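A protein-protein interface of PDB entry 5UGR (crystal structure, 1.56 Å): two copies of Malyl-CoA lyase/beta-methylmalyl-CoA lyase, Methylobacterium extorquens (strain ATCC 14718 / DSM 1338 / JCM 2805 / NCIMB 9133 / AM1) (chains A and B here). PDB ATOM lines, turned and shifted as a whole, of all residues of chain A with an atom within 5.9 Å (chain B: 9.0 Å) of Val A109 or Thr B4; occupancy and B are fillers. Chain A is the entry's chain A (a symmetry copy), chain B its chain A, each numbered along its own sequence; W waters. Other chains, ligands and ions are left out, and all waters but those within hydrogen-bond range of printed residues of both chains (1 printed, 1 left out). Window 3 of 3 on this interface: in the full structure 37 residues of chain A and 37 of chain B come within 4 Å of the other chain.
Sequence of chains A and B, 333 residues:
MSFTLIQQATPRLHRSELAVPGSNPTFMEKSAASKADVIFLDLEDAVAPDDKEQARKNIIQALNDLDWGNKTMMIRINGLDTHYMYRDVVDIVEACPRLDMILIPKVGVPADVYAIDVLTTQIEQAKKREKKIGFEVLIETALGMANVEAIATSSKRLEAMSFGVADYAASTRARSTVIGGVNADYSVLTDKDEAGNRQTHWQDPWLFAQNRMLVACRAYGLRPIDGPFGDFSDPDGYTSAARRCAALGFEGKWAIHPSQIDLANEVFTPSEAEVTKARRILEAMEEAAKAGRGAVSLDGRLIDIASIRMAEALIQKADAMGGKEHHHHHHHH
Water W1 bridges the side-chain hydroxyl (OH) of Tyr B220 and the side-chain amide oxygen (OD1) of Asn A147.
Of the 12 printed residues of chain A, 5 touch a printed residue of chain B.
Hydrophobic or aromatic side chains of chain A within 4 Å of the printed part of chain B: Val A109 and Leu A143.
Of the 11 printed residues of chain B, 5 touch a printed residue of chain A.
Printed residues of chain B that touch a printed residue of chain A: Ser B2, Phe B3, Thr B4, Ala B219 and Tyr B220.
Hydrophobic or aromatic side chains of chain B that line the printed part of chain A: Phe B3, Ala B219 and Tyr B220.
Among the printed residues, 8 pairs touch across the chains.
Among the printed residues, no Asp or Glu carboxylate lies within 4 Å of a Lys or Arg side-chain nitrogen of the other chain.
Val A109 touches just one residue of chain B: Thr B4 (3.5 Å).
Of chain A, only Val A109 (3.5 Å) and Leu A143 (3.7 Å) come within 4 Å of Thr B4.
Gly A108 touches just one residue of chain B: Ser B2 (3.7 Å).
No residue of chain B comes within 4 Å of Pro A110.
Of the printed residues of chain B, Asn A147 touches Tyr B220.
Of the printed residues of chain A, Tyr B220 touches Leu A143 (3.6 Å) and Asn A147 (3.2 Å).
Leu B5 touches none of the printed residues of chain A.
The nearest printed residue of chain A that does not touch Phe B3 is Gly A108 (6.1 Å).
Gly A108 touches Ser B2 (CA to OG, 3.7 Å).
OG1 of Thr B4 touches CG2 of Val A109, at 3.5 Å.
CD2 of Leu A143 touches O of Thr B4, 3.7 Å away.
CA of Leu A143 touches CB of Ala B219, at 3.7 Å.
Leu A143 touches Tyr B220 (CD1 to CE1, 3.6 Å).
No position is printed for both chains.
Of the 8 pairs that touch across the chains among the printed residues, none has its exchanged pair printed and touching as well.
OG of Ser B2 lies within hydrogen-bond range of OD2 of Asp A112, at 2.7 Å.
The backbone NH of Phe B3 is in hydrogen-bond range of the side-chain carboxylate of Asp A112 (3.1 Å).
The side-chain hydroxyl (OH) of Tyr B220 is in hydrogen-bond range of the side-chain amide nitrogen (ND2) of Asn A147 (3.2 Å).
The side-chain hydroxyl of Ser B2 sits at hydrogen-bond distance from the backbone NH of Thr B4, at 3.0 Å.
The backbone NH (N) of Gly A108 sits at hydrogen-bond distance from the side-chain carboxylate (OD2) of Asp A112.
The backbone carbonyl oxygen of Gly A108 is in hydrogen-bond range of the side-chain amide nitrogen of Asn A147.
The backbone NH (N) of Val A109 lies within hydrogen-bond range of the side-chain carboxylate (OD2) of Asp A112 (3.2 Å).
The backbone carbonyl oxygen of Leu A143 lies within hydrogen-bond range of the side-chain amide nitrogen of Asn A147 (3.0 Å).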
ATOM      1  N   VAL A 107       4.723  31.916   3.985  1.00  0.00           N
ATOM      2  CA  VAL A 107       5.846  31.239   3.293  1.00  0.00           C
ATOM      3  C   VAL A 107       5.663  29.710   3.387  1.00  0.00           C
ATOM      4  O   VAL A 107       5.349  29.168   4.451  1.00  0.00           O
ATOM      5  CB  VAL A 107       7.219  31.657   3.883  1.00  0.00           C
ATOM      6  CG1 VAL A 107       8.384  30.875   3.272  1.00  0.00           C
ATOM      7  CG2 VAL A 107       7.417  33.152   3.661  1.00  0.00           C
ATOM      8  N   GLY A 108       5.823  29.049   2.248  1.00  0.00           N
ATOM      9  CA  GLY A 108       5.573  27.607   2.158  1.00  0.00           C
ATOM     10  C   GLY A 108       6.808  26.782   1.925  1.00  0.00           C
ATOM     11  O   GLY A 108       6.910  25.687   2.442  1.00  0.00           O
ATOM     12  N   VAL A 109       7.728  27.284   1.119  1.00  0.00           N
ATOM     13  CA  VAL A 109       8.934  26.563   0.715  1.00  0.00           C
ATOM     14  C   VAL A 109      10.113  27.548   0.620  1.00  0.00           C
ATOM     15  O   VAL A 109       9.921  28.762   0.458  1.00  0.00           O
ATOM     16  CB  VAL A 109       8.769  25.824  -0.630  1.00  0.00           C
ATOM     17  CG1 VAL A 109       7.677  24.787  -0.555  1.00  0.00           C
ATOM     18  CG2 VAL A 109       8.477  26.778  -1.785  1.00  0.00           C
ATOM     19  N   PRO A 110      11.353  27.066   0.718  1.00  0.00           N
ATOM     20  CA  PRO A 110      12.515  27.954   0.655  1.00  0.00           C
ATOM     21  C   PRO A 110      12.568  28.845  -0.604  1.00  0.00           C
ATOM     22  O   PRO A 110      12.996  30.006  -0.535  1.00  0.00           O
ATOM     23  CB  PRO A 110      13.705  27.032   0.762  1.00  0.00           C
ATOM     24  CG  PRO A 110      13.222  25.742   1.083  1.00  0.00           C
ATOM     25  CD  PRO A 110      11.737  25.687   1.046  1.00  0.00           C
ATOM     26  N   ALA A 111      12.100  28.315  -1.733  1.00  0.00           N
ATOM     27  CA  ALA A 111      12.174  29.078  -2.990  1.00  0.00           C
ATOM     28  C   ALA A 111      11.275  30.320  -2.939  1.00  0.00           C
ATOM     29  O   ALA A 111      11.528  31.288  -3.698  1.00  0.00           O
ATOM     30  CB  ALA A 111      11.805  28.212  -4.190  1.00  0.00           C
ATOM     31  N   ASP A 112      10.251  30.340  -2.063  1.00  0.00           N
ATOM     32  CA  ASP A 112       9.463  31.569  -1.884  1.00  0.00           C
ATOM     33  C   ASP A 112      10.389  32.701  -1.428  1.00  0.00           C
ATOM     34  O   ASP A 112      10.304  33.866  -1.895  1.00  0.00           O
ATOM     35  CB  ASP A 112       8.343  31.372  -0.835  1.00  0.00           C
ATOM     36  CG  ASP A 112       7.174  30.487  -1.315  1.00  0.00           C
ATOM     37  OD1 ASP A 112       6.852  30.545  -2.513  1.00  0.00           O
ATOM     38  OD2 ASP A 112       6.615  29.833  -0.390  1.00  0.00           O
ATOM     39  N   VAL A 113      11.257  32.386  -0.493  1.00  0.00           N
ATOM     40  CA  VAL A 113      12.180  33.384   0.071  1.00  0.00           C
ATOM     41  C   VAL A 113      13.237  33.780  -0.963  1.00  0.00           C
ATOM     42  O   VAL A 113      13.552  34.969  -1.122  1.00  0.00           O
ATOM     43  CB  VAL A 113      12.800  32.901   1.370  1.00  0.00           C
ATOM     44  CG1 VAL A 113      13.666  34.008   1.995  1.00  0.00           C
ATOM     45  CG2 VAL A 113      11.747  32.481   2.363  1.00  0.00           C
ATOM     46  N   LEU A 143       1.563  24.184   5.322  1.00  0.00           N
ATOM     47  CA  LEU A 143       2.661  24.007   4.353  1.00  0.00           C
ATOM     48  C   LEU A 143       3.953  24.577   4.853  1.00  0.00           C
ATOM     49  O   LEU A 143       5.013  23.902   4.783  1.00  0.00           O
ATOM     50  CB  LEU A 143       2.320  24.599   2.968  1.00  0.00           C
ATOM     51  CG  LEU A 143       3.315  24.367   1.798  1.00  0.00           C
ATOM     52  CD1 LEU A 143       3.512  22.899   1.477  1.00  0.00           C
ATOM     53  CD2 LEU A 143       2.883  25.172   0.585  1.00  0.00           C
ATOM     54  N   GLY A 144       3.919  25.822   5.329  1.00  0.00           N
ATOM     55  CA  GLY A 144       5.130  26.405   5.868  1.00  0.00           C
ATOM     56  C   GLY A 144       5.657  25.640   7.081  1.00  0.00           C
ATOM     57  O   GLY A 144       6.875  25.436   7.231  1.00  0.00           O
ATOM     58  N   ASN A 147       7.665  22.621   6.181  1.00  0.00           N
ATOM     59  CA  ASN A 147       8.905  22.933   5.535  1.00  0.00           C
ATOM     60  C   ASN A 147       9.754  23.918   6.344  1.00  0.00           C
ATOM     61  O   ASN A 147      10.707  24.495   5.811  1.00  0.00           O
ATOM     62  CB  ASN A 147       8.649  23.455   4.116  1.00  0.00           C
ATOM     63  CG  ASN A 147       8.078  22.378   3.236  1.00  0.00           C
ATOM     64  OD1 ASN A 147       8.796  21.451   2.868  1.00  0.00           O
ATOM     65  ND2 ASN A 147       6.843  22.472   2.918  1.00  0.00           N
ATOM     66  N   ILE A 151      13.010  26.220   5.266  1.00  0.00           N
ATOM     67  CA  ILE A 151      12.837  27.685   5.103  1.00  0.00           C
ATOM     68  C   ILE A 151      13.881  28.435   5.911  1.00  0.00           C
ATOM     69  O   ILE A 151      14.359  29.492   5.509  1.00  0.00           O
ATOM     70  CB  ILE A 151      11.383  28.090   5.488  1.00  0.00           C
ATOM     71  CG1 ILE A 151      10.376  27.524   4.459  1.00  0.00           C
ATOM     72  CG2 ILE A 151      11.239  29.597   5.617  1.00  0.00           C
ATOM     73  CD1 ILE A 151       8.940  27.487   4.949  1.00  0.00           C
ATOM     74  N   SER A 154      17.041  29.558   3.967  1.00  0.00           N
ATOM     75  CA  SER A 154      16.739  29.934   2.585  1.00  0.00           C
ATOM     76  C   SER A 154      17.311  31.247   2.088  1.00  0.00           C
ATOM     77  O   SER A 154      17.194  31.493   0.878  1.00  0.00           O
ATOM     78  CB  SER A 154      15.221  29.981   2.428  1.00  0.00           C
ATOM     79  OG  SER A 154      14.601  30.939   3.258  1.00  0.00           O
ATOM     80  N   SER B   2       2.174  31.424  -0.215  1.00  0.00           N
ATOM     81  CA  SER B   2       3.196  30.711  -0.993  1.00  0.00           C
ATOM     82  C   SER B   2       2.859  30.732  -2.475  1.00  0.00           C
ATOM     83  O   SER B   2       1.671  30.679  -2.872  1.00  0.00           O
ATOM     84  CB  SER B   2       3.326  29.258  -0.522  1.00  0.00           C
ATOM     85  OG  SER B   2       4.391  28.576  -1.199  1.00  0.00           O
ATOM     86  N   PHE B   3       3.900  30.685  -3.290  1.00  0.00           N
ATOM     87  CA  PHE B   3       3.723  30.422  -4.710  1.00  0.00           C
ATOM     88  C   PHE B   3       3.474  28.921  -5.027  1.00  0.00           C
ATOM     89  O   PHE B   3       3.055  28.576  -6.151  1.00  0.00           O
ATOM     90  CB  PHE B   3       4.914  30.962  -5.496  1.00  0.00           C
ATOM     91  CG  PHE B   3       4.739  30.878  -7.004  1.00  0.00           C
ATOM     92  CD1 PHE B   3       3.827  31.734  -7.639  1.00  0.00           C
ATOM     93  CD2 PHE B   3       5.502  30.063  -7.773  1.00  0.00           C
ATOM     94  CE1 PHE B   3       3.675  31.687  -9.005  1.00  0.00           C
ATOM     95  CE2 PHE B   3       5.336  29.992  -9.142  1.00  0.00           C
ATOM     96  CZ  PHE B   3       4.437  30.814  -9.767  1.00  0.00           C
ATOM     97  N   THR B   4       3.829  28.036  -4.072  1.00  0.00           N
ATOM     98  CA  THR B   4       3.577  26.614  -4.200  1.00  0.00           C
ATOM     99  C   THR B   4       2.183  26.288  -3.742  1.00  0.00           C
ATOM    100  O   THR B   4       1.811  26.596  -2.613  1.00  0.00           O
ATOM    101  CB  THR B   4       4.655  25.852  -3.423  1.00  0.00           C
ATOM    102  OG1 THR B   4       5.949  26.084  -4.035  1.00  0.00           O
ATOM    103  CG2 THR B   4       4.418  24.357  -3.451  1.00  0.00           C
ATOM    104  N   LEU B   5       1.416  25.640  -4.629  1.00  0.00           N
ATOM    105  CA  LEU B   5      -0.012  25.352  -4.412  1.00  0.00           C
ATOM    106  C   LEU B   5      -0.260  23.869  -4.455  1.00  0.00           C
ATOM    107  O   LEU B   5       0.211  23.177  -5.419  1.00  0.00           O
ATOM    108  CB  LEU B   5      -0.792  26.041  -5.509  1.00  0.00           C
ATOM    109  CG  LEU B   5      -2.264  25.911  -5.531  1.00  0.00           C
ATOM    110  CD1 LEU B   5      -2.859  26.518  -4.280  1.00  0.00           C
ATOM    111  CD2 LEU B   5      -2.842  26.534  -6.798  1.00  0.00           C
ATOM    112  N   ILE B   6      -1.019  23.396  -3.461  1.00  0.00           N
ATOM    113  CA  ILE B   6      -1.376  21.967  -3.328  1.00  0.00           C
ATOM    114  C   ILE B   6      -2.897  21.749  -3.698  1.00  0.00           C
ATOM    115  O   ILE B   6      -3.756  22.624  -3.536  1.00  0.00           O
ATOM    116  CB  ILE B   6      -1.029  21.467  -1.888  1.00  0.00           C
ATOM    117  CG1 ILE B   6       0.412  21.876  -1.391  1.00  0.00           C
ATOM    118  CG2 ILE B   6      -1.099  19.945  -1.843  1.00  0.00           C
ATOM    119  CD1 ILE B   6       1.665  21.403  -2.090  1.00  0.00           C
ATOM    120  N   GLN B   7      -3.171  20.714  -4.417  1.00  0.00           N
ATOM    121  CA  GLN B   7      -4.561  20.349  -4.674  1.00  0.00           C
ATOM    122  C   GLN B   7      -5.162  19.474  -3.542  1.00  0.00           C
ATOM    123  O   GLN B   7      -4.497  18.569  -3.116  1.00  0.00           O
ATOM    124  CB  GLN B   7      -4.615  19.594  -5.971  1.00  0.00           C
ATOM    125  CG  GLN B   7      -6.028  19.323  -6.448  1.00  0.00           C
ATOM    126  CD  GLN B   7      -5.983  18.697  -7.813  1.00  0.00           C
ATOM    127  OE1 GLN B   7      -5.279  19.180  -8.693  1.00  0.00           O
ATOM    128  NE2 GLN B   7      -6.686  17.608  -7.991  1.00  0.00           N
ATOM    129  N   ALA B 219      -0.865  20.266   5.253  1.00  0.00           N
ATOM    130  CA  ALA B 219       0.044  20.846   4.290  1.00  0.00           C
ATOM    131  C   ALA B 219      -0.262  20.326   2.891  1.00  0.00           C
ATOM    132  O   ALA B 219      -0.202  21.096   1.940  1.00  0.00           O
ATOM    133  CB  ALA B 219       1.466  20.503   4.635  1.00  0.00           C
ATOM    134  N   TYR B 220      -0.620  19.044   2.784  1.00  0.00           N
ATOM    135  CA  TYR B 220      -0.617  18.345   1.513  1.00  0.00           C
ATOM    136  C   TYR B 220      -2.009  17.859   1.055  1.00  0.00           C
ATOM    137  O   TYR B 220      -2.086  17.045   0.102  1.00  0.00           O
ATOM    138  CB  TYR B 220       0.465  17.283   1.513  1.00  0.00           C
ATOM    139  CG  TYR B 220       1.842  17.888   1.690  1.00  0.00           C
ATOM    140  CD1 TYR B 220       2.340  18.806   0.758  1.00  0.00           C
ATOM    141  CD2 TYR B 220       2.630  17.574   2.769  1.00  0.00           C
ATOM    142  CE1 TYR B 220       3.581  19.378   0.935  1.00  0.00           C
ATOM    143  CE2 TYR B 220       3.887  18.133   2.963  1.00  0.00           C
ATOM    144  CZ  TYR B 220       4.377  19.026   2.028  1.00  0.00           C
ATOM    145  OH  TYR B 220       5.615  19.622   2.194  1.00  0.00           O
ATOM    146  N   ILE B 305      -6.339  31.743  -2.704  1.00  0.00           N
ATOM    147  CA  ILE B 305      -6.727  30.488  -3.326  1.00  0.00           C
ATOM    148  C   ILE B 305      -6.657  29.314  -2.338  1.00  0.00           C
ATOM    149  O   ILE B 305      -7.528  28.438  -2.368  1.00  0.00           O
ATOM    150  CB  ILE B 305      -5.923  30.227  -4.617  1.00  0.00           C
ATOM    151  CG1 ILE B 305      -6.419  29.002  -5.358  1.00  0.00           C
ATOM    152  CG2 ILE B 305      -4.394  30.118  -4.342  1.00  0.00           C
ATOM    153  CD1 ILE B 305      -5.846  28.871  -6.756  1.00  0.00           C
ATOM    154  N   ALA B 306      -5.653  29.268  -1.442  1.00  0.00           N
ATOM    155  CA  ALA B 306      -5.645  28.161  -0.484  1.00  0.00           C
ATOM    156  C   ALA B 306      -6.894  28.147   0.385  1.00  0.00           C
ATOM    157  O   ALA B 306      -7.488  27.102   0.655  1.00  0.00           O
ATOM    158  CB  ALA B 306      -4.393  28.287   0.384  1.00  0.00           C
ATOM    159  N   ARG B 309      -9.940  27.000  -1.600  1.00  0.00           N
ATOM    160  CA  ARG B 309      -9.946  25.551  -1.700  1.00  0.00           C
ATOM    161  C   ARG B 309     -10.391  24.854  -0.437  1.00  0.00           C
ATOM    162  O   ARG B 309     -11.133  23.852  -0.511  1.00  0.00           O
ATOM    163  CB  ARG B 309      -8.623  25.013  -2.255  1.00  0.00           C
ATOM    164  CG  ARG B 309      -8.339  25.458  -3.667  1.00  0.00           C
ATOM    165  CD  ARG B 309      -6.978  25.072  -4.223  1.00  0.00           C
ATOM    166  NE  ARG B 309      -6.931  25.253  -5.682  1.00  0.00           N
ATOM    167  CZ  ARG B 309      -6.074  24.652  -6.482  1.00  0.00           C
ATOM    168  NH1 ARG B 309      -5.100  23.852  -5.984  1.00  0.00           N
ATOM    169  NH2 ARG B 309      -6.161  24.903  -7.773  1.00  0.00           N
HETATM  170  O   HOH W   1       7.185  18.616   4.121  1.00  0.00           O
